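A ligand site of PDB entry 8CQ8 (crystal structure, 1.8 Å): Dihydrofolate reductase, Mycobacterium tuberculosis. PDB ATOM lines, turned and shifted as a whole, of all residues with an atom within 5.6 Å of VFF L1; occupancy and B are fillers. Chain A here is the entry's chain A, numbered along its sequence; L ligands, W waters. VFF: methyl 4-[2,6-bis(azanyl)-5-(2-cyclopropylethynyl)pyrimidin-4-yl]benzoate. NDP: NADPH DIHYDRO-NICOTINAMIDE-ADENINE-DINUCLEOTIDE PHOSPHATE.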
ATOM      1  N   ILE A   7      21.252 -10.378   8.069  1.00  0.00           N
ATOM      2  CA  ILE A   7      22.209 -10.562   9.147  1.00  0.00           C
ATOM      3  C   ILE A   7      21.654 -11.584  10.135  1.00  0.00           C
ATOM      4  O   ILE A   7      20.474 -11.504  10.512  1.00  0.00           O
ATOM      5  CB  ILE A   7      22.536  -9.209   9.813  1.00  0.00           C
ATOM      6  CG1 ILE A   7      23.576  -9.392  10.919  1.00  0.00           C
ATOM      7  CG2 ILE A   7      21.263  -8.493  10.287  1.00  0.00           C
ATOM      8  CD1 ILE A   7      24.321  -8.134  11.285  1.00  0.00           C
ATOM      9  N   TRP A   8      22.478 -12.560  10.538  1.00  0.00           N
ATOM     10  CA  TRP A   8      22.063 -13.592  11.492  1.00  0.00           C
ATOM     11  C   TRP A   8      23.290 -14.189  12.153  1.00  0.00           C
ATOM     12  O   TRP A   8      24.397 -14.124  11.620  1.00  0.00           O
ATOM     13  CB  TRP A   8      21.272 -14.718  10.826  1.00  0.00           C
ATOM     14  CG  TRP A   8      22.063 -15.690   9.974  1.00  0.00           C
ATOM     15  CD1 TRP A   8      22.879 -16.709  10.400  1.00  0.00           C
ATOM     16  CD2 TRP A   8      22.042 -15.774   8.542  1.00  0.00           C
ATOM     17  NE1 TRP A   8      23.387 -17.391   9.324  1.00  0.00           N
ATOM     18  CE2 TRP A   8      22.890 -16.843   8.176  1.00  0.00           C
ATOM     19  CE3 TRP A   8      21.405 -15.050   7.538  1.00  0.00           C
ATOM     20  CZ2 TRP A   8      23.119 -17.190   6.843  1.00  0.00           C
ATOM     21  CZ3 TRP A   8      21.623 -15.390   6.232  1.00  0.00           C
ATOM     22  CH2 TRP A   8      22.474 -16.452   5.887  1.00  0.00           C
ATOM     23  N   ALA A   9      23.060 -14.816  13.313  1.00  0.00           N
ATOM     24  CA  ALA A   9      24.071 -15.609  14.006  1.00  0.00           C
ATOM     25  C   ALA A   9      23.596 -17.049  14.022  1.00  0.00           C
ATOM     26  O   ALA A   9      22.440 -17.316  14.311  1.00  0.00           O
ATOM     27  CB  ALA A   9      24.298 -15.115  15.424  1.00  0.00           C
ATOM     28  N   ILE A  22      17.278 -17.708  21.550  1.00  0.00           N
ATOM     29  CA  ILE A  22      18.605 -18.035  21.021  1.00  0.00           C
ATOM     30  C   ILE A  22      19.399 -18.753  22.108  1.00  0.00           C
ATOM     31  O   ILE A  22      19.584 -18.203  23.195  1.00  0.00           O
ATOM     32  CB  ILE A  22      19.322 -16.764  20.561  1.00  0.00           C
ATOM     33  CG1 ILE A  22      18.440 -16.049  19.537  1.00  0.00           C
ATOM     34  CG2 ILE A  22      20.661 -17.105  19.959  1.00  0.00           C
ATOM     35  CD1 ILE A  22      18.887 -14.675  19.187  1.00  0.00           C
ATOM     36  N   ARG A  25      24.535 -16.205  23.839  1.00  0.00           N
ATOM     37  CA  ARG A  25      24.588 -14.746  23.789  1.00  0.00           C
ATOM     38  C   ARG A  25      26.054 -14.340  23.740  1.00  0.00           C
ATOM     39  O   ARG A  25      26.803 -14.638  24.676  1.00  0.00           O
ATOM     40  CB  ARG A  25      23.903 -14.084  24.990  1.00  0.00           C
ATOM     41  CG  ARG A  25      23.607 -12.606  24.728  1.00  0.00           C
ATOM     42  CD  ARG A  25      22.515 -12.073  25.647  1.00  0.00           C
ATOM     43  NE  ARG A  25      21.187 -12.601  25.357  1.00  0.00           N
ATOM     44  CZ  ARG A  25      20.124 -12.343  26.123  1.00  0.00           C
ATOM     45  NH1 ARG A  25      20.246 -11.561  27.178  1.00  0.00           N
ATOM     46  NH2 ARG A  25      18.939 -12.875  25.822  1.00  0.00           N
ATOM     47  N   ASP A  29      28.899 -10.259  19.169  1.00  0.00           N
ATOM     48  CA  ASP A  29      27.984 -10.339  18.032  1.00  0.00           C
ATOM     49  C   ASP A  29      26.892  -9.271  18.113  1.00  0.00           C
ATOM     50  O   ASP A  29      26.410  -8.813  17.074  1.00  0.00           O
ATOM     51  CB  ASP A  29      27.341 -11.714  17.965  1.00  0.00           C
ATOM     52  CG  ASP A  29      26.282 -11.786  16.917  1.00  0.00           C
ATOM     53  OD1 ASP A  29      26.639 -11.757  15.725  1.00  0.00           O
ATOM     54  OD2 ASP A  29      25.085 -11.818  17.273  1.00  0.00           O
ATOM     55  N   GLN A  30      26.489  -8.886  19.320  1.00  0.00           N
ATOM     56  CA  GLN A  30      25.492  -7.834  19.455  1.00  0.00           C
ATOM     57  C   GLN A  30      26.028  -6.498  18.950  1.00  0.00           C
ATOM     58  O   GLN A  30      25.338  -5.757  18.248  1.00  0.00           O
ATOM     59  CB  GLN A  30      25.055  -7.701  20.905  1.00  0.00           C
ATOM     60  CG  GLN A  30      24.225  -6.458  21.085  1.00  0.00           C
ATOM     61  CD  GLN A  30      23.894  -6.184  22.528  1.00  0.00           C
ATOM     62  OE1 GLN A  30      24.364  -6.864  23.436  1.00  0.00           O
ATOM     63  NE2 GLN A  30      23.049  -5.182  22.743  1.00  0.00           N
ATOM     64  N   HIS A  32      28.565  -6.103  16.734  1.00  0.00           N
ATOM     65  CA  HIS A  32      28.624  -6.320  15.289  1.00  0.00           C
ATOM     66  C   HIS A  32      27.261  -6.075  14.636  1.00  0.00           C
ATOM     67  O   HIS A  32      27.168  -5.448  13.571  1.00  0.00           O
ATOM     68  CB  HIS A  32      29.090  -7.746  15.024  1.00  0.00           C
ATOM     69  CG  HIS A  32      29.092  -8.143  13.582  1.00  0.00           C
ATOM     70  ND1 HIS A  32      29.928  -7.584  12.655  1.00  0.00           N
ATOM     71  CD2 HIS A  32      28.341  -9.052  12.922  1.00  0.00           C
ATOM     72  CE1 HIS A  32      29.717  -8.143  11.479  1.00  0.00           C
ATOM     73  NE2 HIS A  32      28.738  -9.023  11.612  1.00  0.00           N
ATOM     74  N   PHE A  33      26.196  -6.607  15.240  1.00  0.00           N
ATOM     75  CA  PHE A  33      24.861  -6.438  14.691  1.00  0.00           C
ATOM     76  C   PHE A  33      24.448  -4.973  14.681  1.00  0.00           C
ATOM     77  O   PHE A  33      23.973  -4.452  13.665  1.00  0.00           O
ATOM     78  CB  PHE A  33      23.883  -7.295  15.488  1.00  0.00           C
ATOM     79  CG  PHE A  33      22.441  -6.978  15.241  1.00  0.00           C
ATOM     80  CD1 PHE A  33      21.753  -7.525  14.166  1.00  0.00           C
ATOM     81  CD2 PHE A  33      21.753  -6.135  16.113  1.00  0.00           C
ATOM     82  CE1 PHE A  33      20.423  -7.224  13.943  1.00  0.00           C
ATOM     83  CE2 PHE A  33      20.422  -5.827  15.902  1.00  0.00           C
ATOM     84  CZ  PHE A  33      19.747  -6.375  14.822  1.00  0.00           C
ATOM     85  N   MET A  44      11.857  -7.698  10.529  1.00  0.00           N
ATOM     86  CA  MET A  44      11.838  -8.892  11.366  1.00  0.00           C
ATOM     87  C   MET A  44      10.462  -9.550  11.289  1.00  0.00           C
ATOM     88  O   MET A  44       9.445  -8.884  11.066  1.00  0.00           O
ATOM     89  CB  MET A  44      12.213  -8.538  12.817  1.00  0.00           C
ATOM     90  CG  MET A  44      11.111  -7.896  13.648  1.00  0.00           C
ATOM     91  SD  MET A  44      11.624  -7.110  15.218  1.00  0.00           S
ATOM     92  CE  MET A  44      12.488  -5.648  14.646  1.00  0.00           C
ATOM     93  N   THR A  48       9.974 -12.927  15.903  1.00  0.00           N
ATOM     94  CA  THR A  48      11.184 -12.253  16.357  1.00  0.00           C
ATOM     95  C   THR A  48      10.857 -10.989  17.155  1.00  0.00           C
ATOM     96  O   THR A  48      11.447 -10.739  18.212  1.00  0.00           O
ATOM     97  CB  THR A  48      12.061 -11.959  15.150  1.00  0.00           C
ATOM     98  OG1 THR A  48      12.464 -13.200  14.561  1.00  0.00           O
ATOM     99  CG2 THR A  48      13.308 -11.244  15.578  1.00  0.00           C
ATOM    100  N   SER A  51      10.060 -11.941  20.469  1.00  0.00           N
ATOM    101  CA  SER A  51      11.219 -12.366  21.261  1.00  0.00           C
ATOM    102  C   SER A  51      11.951 -11.200  21.914  1.00  0.00           C
ATOM    103  O   SER A  51      12.881 -11.436  22.692  1.00  0.00           O
ATOM    104  CB  SER A  51      12.205 -13.161  20.385  1.00  0.00           C
ATOM    105  OG  SER A  51      13.087 -12.306  19.666  1.00  0.00           O
ATOM    106  N   LEU A  52      11.557  -9.941  21.638  1.00  0.00           N
ATOM    107  CA  LEU A  52      12.203  -8.781  22.242  1.00  0.00           C
ATOM    108  C   LEU A  52      11.370  -8.276  23.414  1.00  0.00           C
ATOM    109  O   LEU A  52      10.154  -8.122  23.272  1.00  0.00           O
ATOM    110  CB  LEU A  52      12.365  -7.657  21.235  1.00  0.00           C
ATOM    111  CG  LEU A  52      13.237  -7.857  19.987  1.00  0.00           C
ATOM    112  CD1 LEU A  52      12.787  -6.876  18.913  1.00  0.00           C
ATOM    113  CD2 LEU A  52      14.737  -7.697  20.260  1.00  0.00           C
ATOM    114  N   LEU A  59      14.191  -1.172  18.389  1.00  0.00           N
ATOM    115  CA  LEU A  59      15.638  -1.023  18.466  1.00  0.00           C
ATOM    116  C   LEU A  59      16.026   0.406  18.102  1.00  0.00           C
ATOM    117  O   LEU A  59      15.582   0.917  17.071  1.00  0.00           O
ATOM    118  CB  LEU A  59      16.310  -2.062  17.554  1.00  0.00           C
ATOM    119  CG  LEU A  59      16.334  -3.544  17.954  1.00  0.00           C
ATOM    120  CD1 LEU A  59      14.970  -4.109  18.276  1.00  0.00           C
ATOM    121  CD2 LEU A  59      16.957  -4.390  16.846  1.00  0.00           C
ATOM    122  N   VAL A  95      17.334  -7.475   6.966  1.00  0.00           N
ATOM    123  CA  VAL A  95      16.445  -8.515   7.478  1.00  0.00           C
ATOM    124  C   VAL A  95      17.105  -9.183   8.674  1.00  0.00           C
ATOM    125  O   VAL A  95      18.169  -9.814   8.525  1.00  0.00           O
ATOM    126  CB  VAL A  95      16.123  -9.529   6.379  1.00  0.00           C
ATOM    127  CG1 VAL A  95      15.369 -10.729   6.950  1.00  0.00           C
ATOM    128  CG2 VAL A  95      15.315  -8.860   5.285  1.00  0.00           C
ATOM    129  N   ILE A  96      16.499  -9.050   9.849  1.00  0.00           N
ATOM    130  CA  ILE A  96      17.169  -9.457  11.080  1.00  0.00           C
ATOM    131  C   ILE A  96      16.566 -10.721  11.698  1.00  0.00           C
ATOM    132  O   ILE A  96      16.915 -11.072  12.838  1.00  0.00           O
ATOM    133  CB  ILE A  96      17.223  -8.307  12.091  1.00  0.00           C
ATOM    134  CG1 ILE A  96      15.858  -7.898  12.610  1.00  0.00           C
ATOM    135  CG2 ILE A  96      17.900  -7.113  11.489  1.00  0.00           C
ATOM    136  CD1 ILE A  96      15.961  -6.998  13.825  1.00  0.00           C
ATOM    137  N   GLY A  97      15.725 -11.443  10.970  1.00  0.00           N
ATOM    138  CA  GLY A  97      15.218 -12.736  11.398  1.00  0.00           C
ATOM    139  C   GLY A  97      13.702 -12.765  11.505  1.00  0.00           C
ATOM    140  O   GLY A  97      13.011 -11.763  11.317  1.00  0.00           O
ATOM    141  N   TYR A 102      13.939 -14.937   6.854  1.00  0.00           N
ATOM    142  CA  TYR A 102      15.170 -15.080   6.062  1.00  0.00           C
ATOM    143  C   TYR A 102      14.869 -15.741   4.745  1.00  0.00           C
ATOM    144  O   TYR A 102      15.342 -15.292   3.692  1.00  0.00           O
ATOM    145  CB  TYR A 102      16.250 -15.887   6.788  1.00  0.00           C
ATOM    146  CG  TYR A 102      16.912 -15.184   7.952  1.00  0.00           C
ATOM    147  CD1 TYR A 102      17.367 -15.905   9.052  1.00  0.00           C
ATOM    148  CD2 TYR A 102      17.027 -13.803   7.978  1.00  0.00           C
ATOM    149  CE1 TYR A 102      17.960 -15.252  10.144  1.00  0.00           C
ATOM    150  CE2 TYR A 102      17.605 -13.156   9.055  1.00  0.00           C
ATOM    151  CZ  TYR A 102      18.070 -13.883  10.127  1.00  0.00           C
ATOM    152  OH  TYR A 102      18.625 -13.227  11.205  1.00  0.00           O
ATOM    153  N   GLU A 113      25.449 -11.109   6.255  1.00  0.00           N
ATOM    154  CA  GLU A 113      26.410 -10.952   7.332  1.00  0.00           C
ATOM    155  C   GLU A 113      26.116 -12.045   8.370  1.00  0.00           C
ATOM    156  O   GLU A 113      25.121 -11.962   9.104  1.00  0.00           O
ATOM    157  CB  GLU A 113      26.309  -9.550   7.946  1.00  0.00           C
ATOM    158  CG  GLU A 113      26.740  -8.455   6.966  1.00  0.00           C
ATOM    159  CD  GLU A 113      28.207  -8.548   6.553  1.00  0.00           C
ATOM    160  OE1 GLU A 113      29.020  -9.075   7.356  1.00  0.00           O
ATOM    161  OE2 GLU A 113      28.530  -8.135   5.402  1.00  0.00           O
ATOM    162  N   THR A 115      27.324 -14.412  11.609  1.00  0.00           N
ATOM    163  CA  THR A 115      28.182 -14.760  12.733  1.00  0.00           C
ATOM    164  C   THR A 115      28.075 -16.261  12.906  1.00  0.00           C
ATOM    165  O   THR A 115      26.974 -16.778  13.097  1.00  0.00           O
ATOM    166  CB  THR A 115      27.752 -14.041  14.019  1.00  0.00           C
ATOM    167  OG1 THR A 115      27.692 -12.633  13.819  1.00  0.00           O
ATOM    168  CG2 THR A 115      28.753 -14.314  15.138  1.00  0.00           C
HETATM  169  C10 VFF L   1      15.823  -9.992  17.782  1.00  0.00           C
HETATM  170  C13 VFF L   1      21.321 -10.592  17.758  1.00  0.00           C
HETATM  171  C15 VFF L   1      20.251 -11.076  19.893  1.00  0.00           C
HETATM  172  C17 VFF L   1      20.731  -9.921  22.043  1.00  0.00           C
HETATM  173  C21 VFF L   1      21.871  -9.368  19.814  1.00  0.00           C
HETATM  174  C22 VFF L   1      22.050  -9.604  18.444  1.00  0.00           C
HETATM  175  C02 VFF L   1      23.033 -11.268  14.563  1.00  0.00           C
HETATM  176  C04 VFF L   1      20.794 -10.901  13.994  1.00  0.00           C
HETATM  177  C06 VFF L   1      20.484 -10.697  15.356  1.00  0.00           C
HETATM  178  C07 VFF L   1      19.168 -10.416  15.733  1.00  0.00           C
HETATM  179  C08 VFF L   1      18.130 -10.122  16.180  1.00  0.00           C
HETATM  180  C09 VFF L   1      16.952  -9.703  16.833  1.00  0.00           C
HETATM  181  C11 VFF L   1      16.081  -8.569  17.224  1.00  0.00           C
HETATM  182  C12 VFF L   1      21.516 -10.818  16.271  1.00  0.00           C
HETATM  183  C14 VFF L   1      20.427 -11.319  18.535  1.00  0.00           C
HETATM  184  C16 VFF L   1      20.968 -10.109  20.572  1.00  0.00           C
HETATM  185  C19 VFF L   1      21.258  -8.880  24.109  1.00  0.00           C
HETATM  186  N01 VFF L   1      24.321 -11.552  14.111  1.00  0.00           N
HETATM  187  N03 VFF L   1      22.077 -11.186  13.566  1.00  0.00           N
HETATM  188  N05 VFF L   1      19.884 -10.837  12.996  1.00  0.00           N
HETATM  189  N23 VFF L   1      22.796 -11.069  15.913  1.00  0.00           N
HETATM  190  O18 VFF L   1      21.501  -9.042  22.714  1.00  0.00           O
HETATM  191  O20 VFF L   1      19.885 -10.513  22.686  1.00  0.00           O
HETATM  192  PA  NDP L   2       9.807 -15.442  12.369  1.00  0.00           P
HETATM  193  O1A NDP L   2      10.666 -14.598  13.251  1.00  0.00           O
HETATM  194  O2A NDP L   2      10.240 -15.882  11.001  1.00  0.00           O
HETATM  195  O5B NDP L   2       8.385 -14.693  12.340  1.00  0.00           O
HETATM  196  C5B NDP L   2       7.539 -15.509  11.664  1.00  0.00           C
HETATM  197  C4B NDP L   2       6.325 -14.674  11.532  1.00  0.00           C
HETATM  198  O4B NDP L   2       6.507 -13.812  10.454  1.00  0.00           O
HETATM  199  C3B NDP L   2       5.096 -15.500  11.243  1.00  0.00           C
HETATM  200  O3B NDP L   2       4.542 -15.969  12.443  1.00  0.00           O
HETATM  201  C2B NDP L   2       4.191 -14.356  10.646  1.00  0.00           C
HETATM  202  O2B NDP L   2       3.748 -13.504  11.537  1.00  0.00           O
HETATM  203  C1B NDP L   2       5.239 -13.569   9.856  1.00  0.00           C
HETATM  204  N9A NDP L   2       5.314 -13.996   8.522  1.00  0.00           N
HETATM  205  C8A NDP L   2       6.039 -15.065   7.993  1.00  0.00           C
HETATM  206  N7A NDP L   2       5.891 -15.185   6.662  1.00  0.00           N
HETATM  207  C5A NDP L   2       5.006 -14.142   6.336  1.00  0.00           C
HETATM  208  C6A NDP L   2       4.473 -13.732   5.130  1.00  0.00           C
HETATM  209  N6A NDP L   2       4.805 -14.426   3.980  1.00  0.00           N
HETATM  210  N1A NDP L   2       3.624 -12.657   5.043  1.00  0.00           N
HETATM  211  C2A NDP L   2       3.356 -12.026   6.237  1.00  0.00           C
HETATM  212  N3A NDP L   2       3.794 -12.295   7.474  1.00  0.00           N
HETATM  213  C4A NDP L   2       4.644 -13.389   7.481  1.00  0.00           C
HETATM  214  O3  NDP L   2       9.622 -16.796  13.273  1.00  0.00           O
HETATM  215  PN  NDP L   2      10.814 -17.841  13.136  1.00  0.00           P
HETATM  216  O1N NDP L   2      10.578 -18.875  14.172  1.00  0.00           O
HETATM  217  O2N NDP L   2      11.198 -18.284  11.746  1.00  0.00           O
HETATM  218  O5D NDP L   2      12.275 -17.156  13.771  1.00  0.00           O
HETATM  219  C5D NDP L   2      12.101 -16.928  15.138  1.00  0.00           C
HETATM  220  C4D NDP L   2      13.264 -17.613  15.856  1.00  0.00           C
HETATM  221  O4D NDP L   2      14.534 -17.205  15.291  1.00  0.00           O
HETATM  222  C3D NDP L   2      13.330 -17.209  17.376  1.00  0.00           C
HETATM  223  O3D NDP L   2      13.951 -18.264  18.057  1.00  0.00           O
HETATM  224  C2D NDP L   2      14.287 -16.061  17.326  1.00  0.00           C
HETATM  225  O2D NDP L   2      14.935 -15.856  18.530  1.00  0.00           O
HETATM  226  C1D NDP L   2      15.308 -16.650  16.348  1.00  0.00           C
HETATM  227  N1N NDP L   2      16.139 -15.570  15.822  1.00  0.00           N
HETATM  228  C2N NDP L   2      17.494 -15.742  15.699  1.00  0.00           C
HETATM  229  C3N NDP L   2      18.279 -14.758  15.155  1.00  0.00           C
HETATM  230  C7N NDP L   2      19.736 -15.009  15.058  1.00  0.00           C
HETATM  231  O7N NDP L   2      20.530 -14.312  14.391  1.00  0.00           O
HETATM  232  N7N NDP L   2      20.245 -16.091  15.788  1.00  0.00           N
HETATM  233  C4N NDP L   2      17.707 -13.479  14.665  1.00  0.00           C
HETATM  234  C5N NDP L   2      16.249 -13.382  14.930  1.00  0.00           C
HETATM  235  C6N NDP L   2      15.548 -14.365  15.469  1.00  0.00           C
HETATM  236  P2B NDP L   2       2.052 -13.855  12.005  1.00  0.00           P
HETATM  237  O1X NDP L   2       1.495 -13.779  10.624  1.00  0.00           O
HETATM  238  O2X NDP L   2       2.229 -15.243  12.650  1.00  0.00           O
HETATM  239  O3X NDP L   2       1.816 -12.687  12.943  1.00  0.00           O
HETATM  240  O   HOH W   1      26.081 -11.279  11.574  1.00  0.00           O
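An oxygen (O1A) of NDP L2 lies within hydrogen-bond range of the side-chain hydroxyl (OG1) of Thr 48, at 2.6 Å.
The side-chain carboxylate of Asp 29 lies within hydrogen-bond range of a nitrogen (N23) of VFF L1.
OH of Tyr 102 is in hydrogen-bond range of N05 of VFF L1 (3.2 Å).
N7N of NDP L2 lies within hydrogen-bond range of O of Ala 9, at 2.9 Å.
O7N of NDP L2 lies within hydrogen-bond range of N of Ala 9 (2.8 Å).
The backbone NH of Trp 8 sits close to a nitrogen (N03) of VFF L1 (3.3 Å).
The backbone NH of Thr 48 lies within hydrogen-bond range of an oxygen (O1A) of NDP L2, at 3.2 Å.
O of Ile 96 sits at hydrogen-bond distance from N05 of VFF L1 (3.0 Å).
The backbone carbonyl oxygen of Ile 7 lies within hydrogen-bond range of a nitrogen (N05) of VFF L1 (2.6 Å).
The backbone NH (N) of Gly 97 lies close to the side-chain hydroxyl (OH) of Tyr 102, 3.4 Å away.
The backbone carbonyl oxygen of Ile 96 is in hydrogen-bond range of the side-chain hydroxyl of Tyr 102 (3.2 Å).
The backbone carbonyl oxygen (O) of Val 95 lies within hydrogen-bond range of the backbone NH (N) of Ile 7, 3.2 Å away.
The backbone NH of Thr 115 sits at hydrogen-bond distance from the backbone carbonyl oxygen of Trp 8, at 2.9 Å.
OG of Ser 51 is in hydrogen-bond range of O of Thr 48 (2.7 Å).
The backbone carbonyl oxygen (O) of Ile 7 sits at hydrogen-bond distance from the side-chain hydroxyl (OH) of Tyr 102 (2.6 Å).
The backbone carbonyl oxygen (O) of Glu 113 sits at hydrogen-bond distance from the backbone NH (N) of Trp 8.
N of Ala 9 touches N01 of VFF L1 (3.6 Å).
Ile 22 touches VFF L1 (CD1 to C14, 3.7 Å).
Arg 25 touches VFF L1.
Gln 30 touches VFF L1.
Phe 33 touches VFF L1 (CD1 to C04, 3.5 Å).
CG2 of Thr 48 touches C10 of VFF L1, 3.6 Å away.
CD2 of Leu 52 touches C11 of VFF L1 (3.4 Å).
Thr 115 touches VFF L1.
Hydrophobic or aromatic side chains within 4 Å of VFF L1: Ile 7, Ala 9, Ile 22, Phe 33, Leu 52 and Ile 96.
Along chain A the residues within 4 Å of VFF L1 span positions 7 to 115.
The nearest printed residue that does not touch VFF L1 is Ser 51 (4.05 Å).
Water W1 lies within hydrogen-bond range of the backbone carbonyl oxygen of Glu 113 (2.7 Å), the side-chain hydroxyl of Thr 115 (3.1 Å), a nitrogen (N01) of VFF L1 (3.1 Å), the backbone carbonyl oxygen of Trp 8 (3.3 Å) and a ring nitrogen (NE2) of His 32 (3.5 Å).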
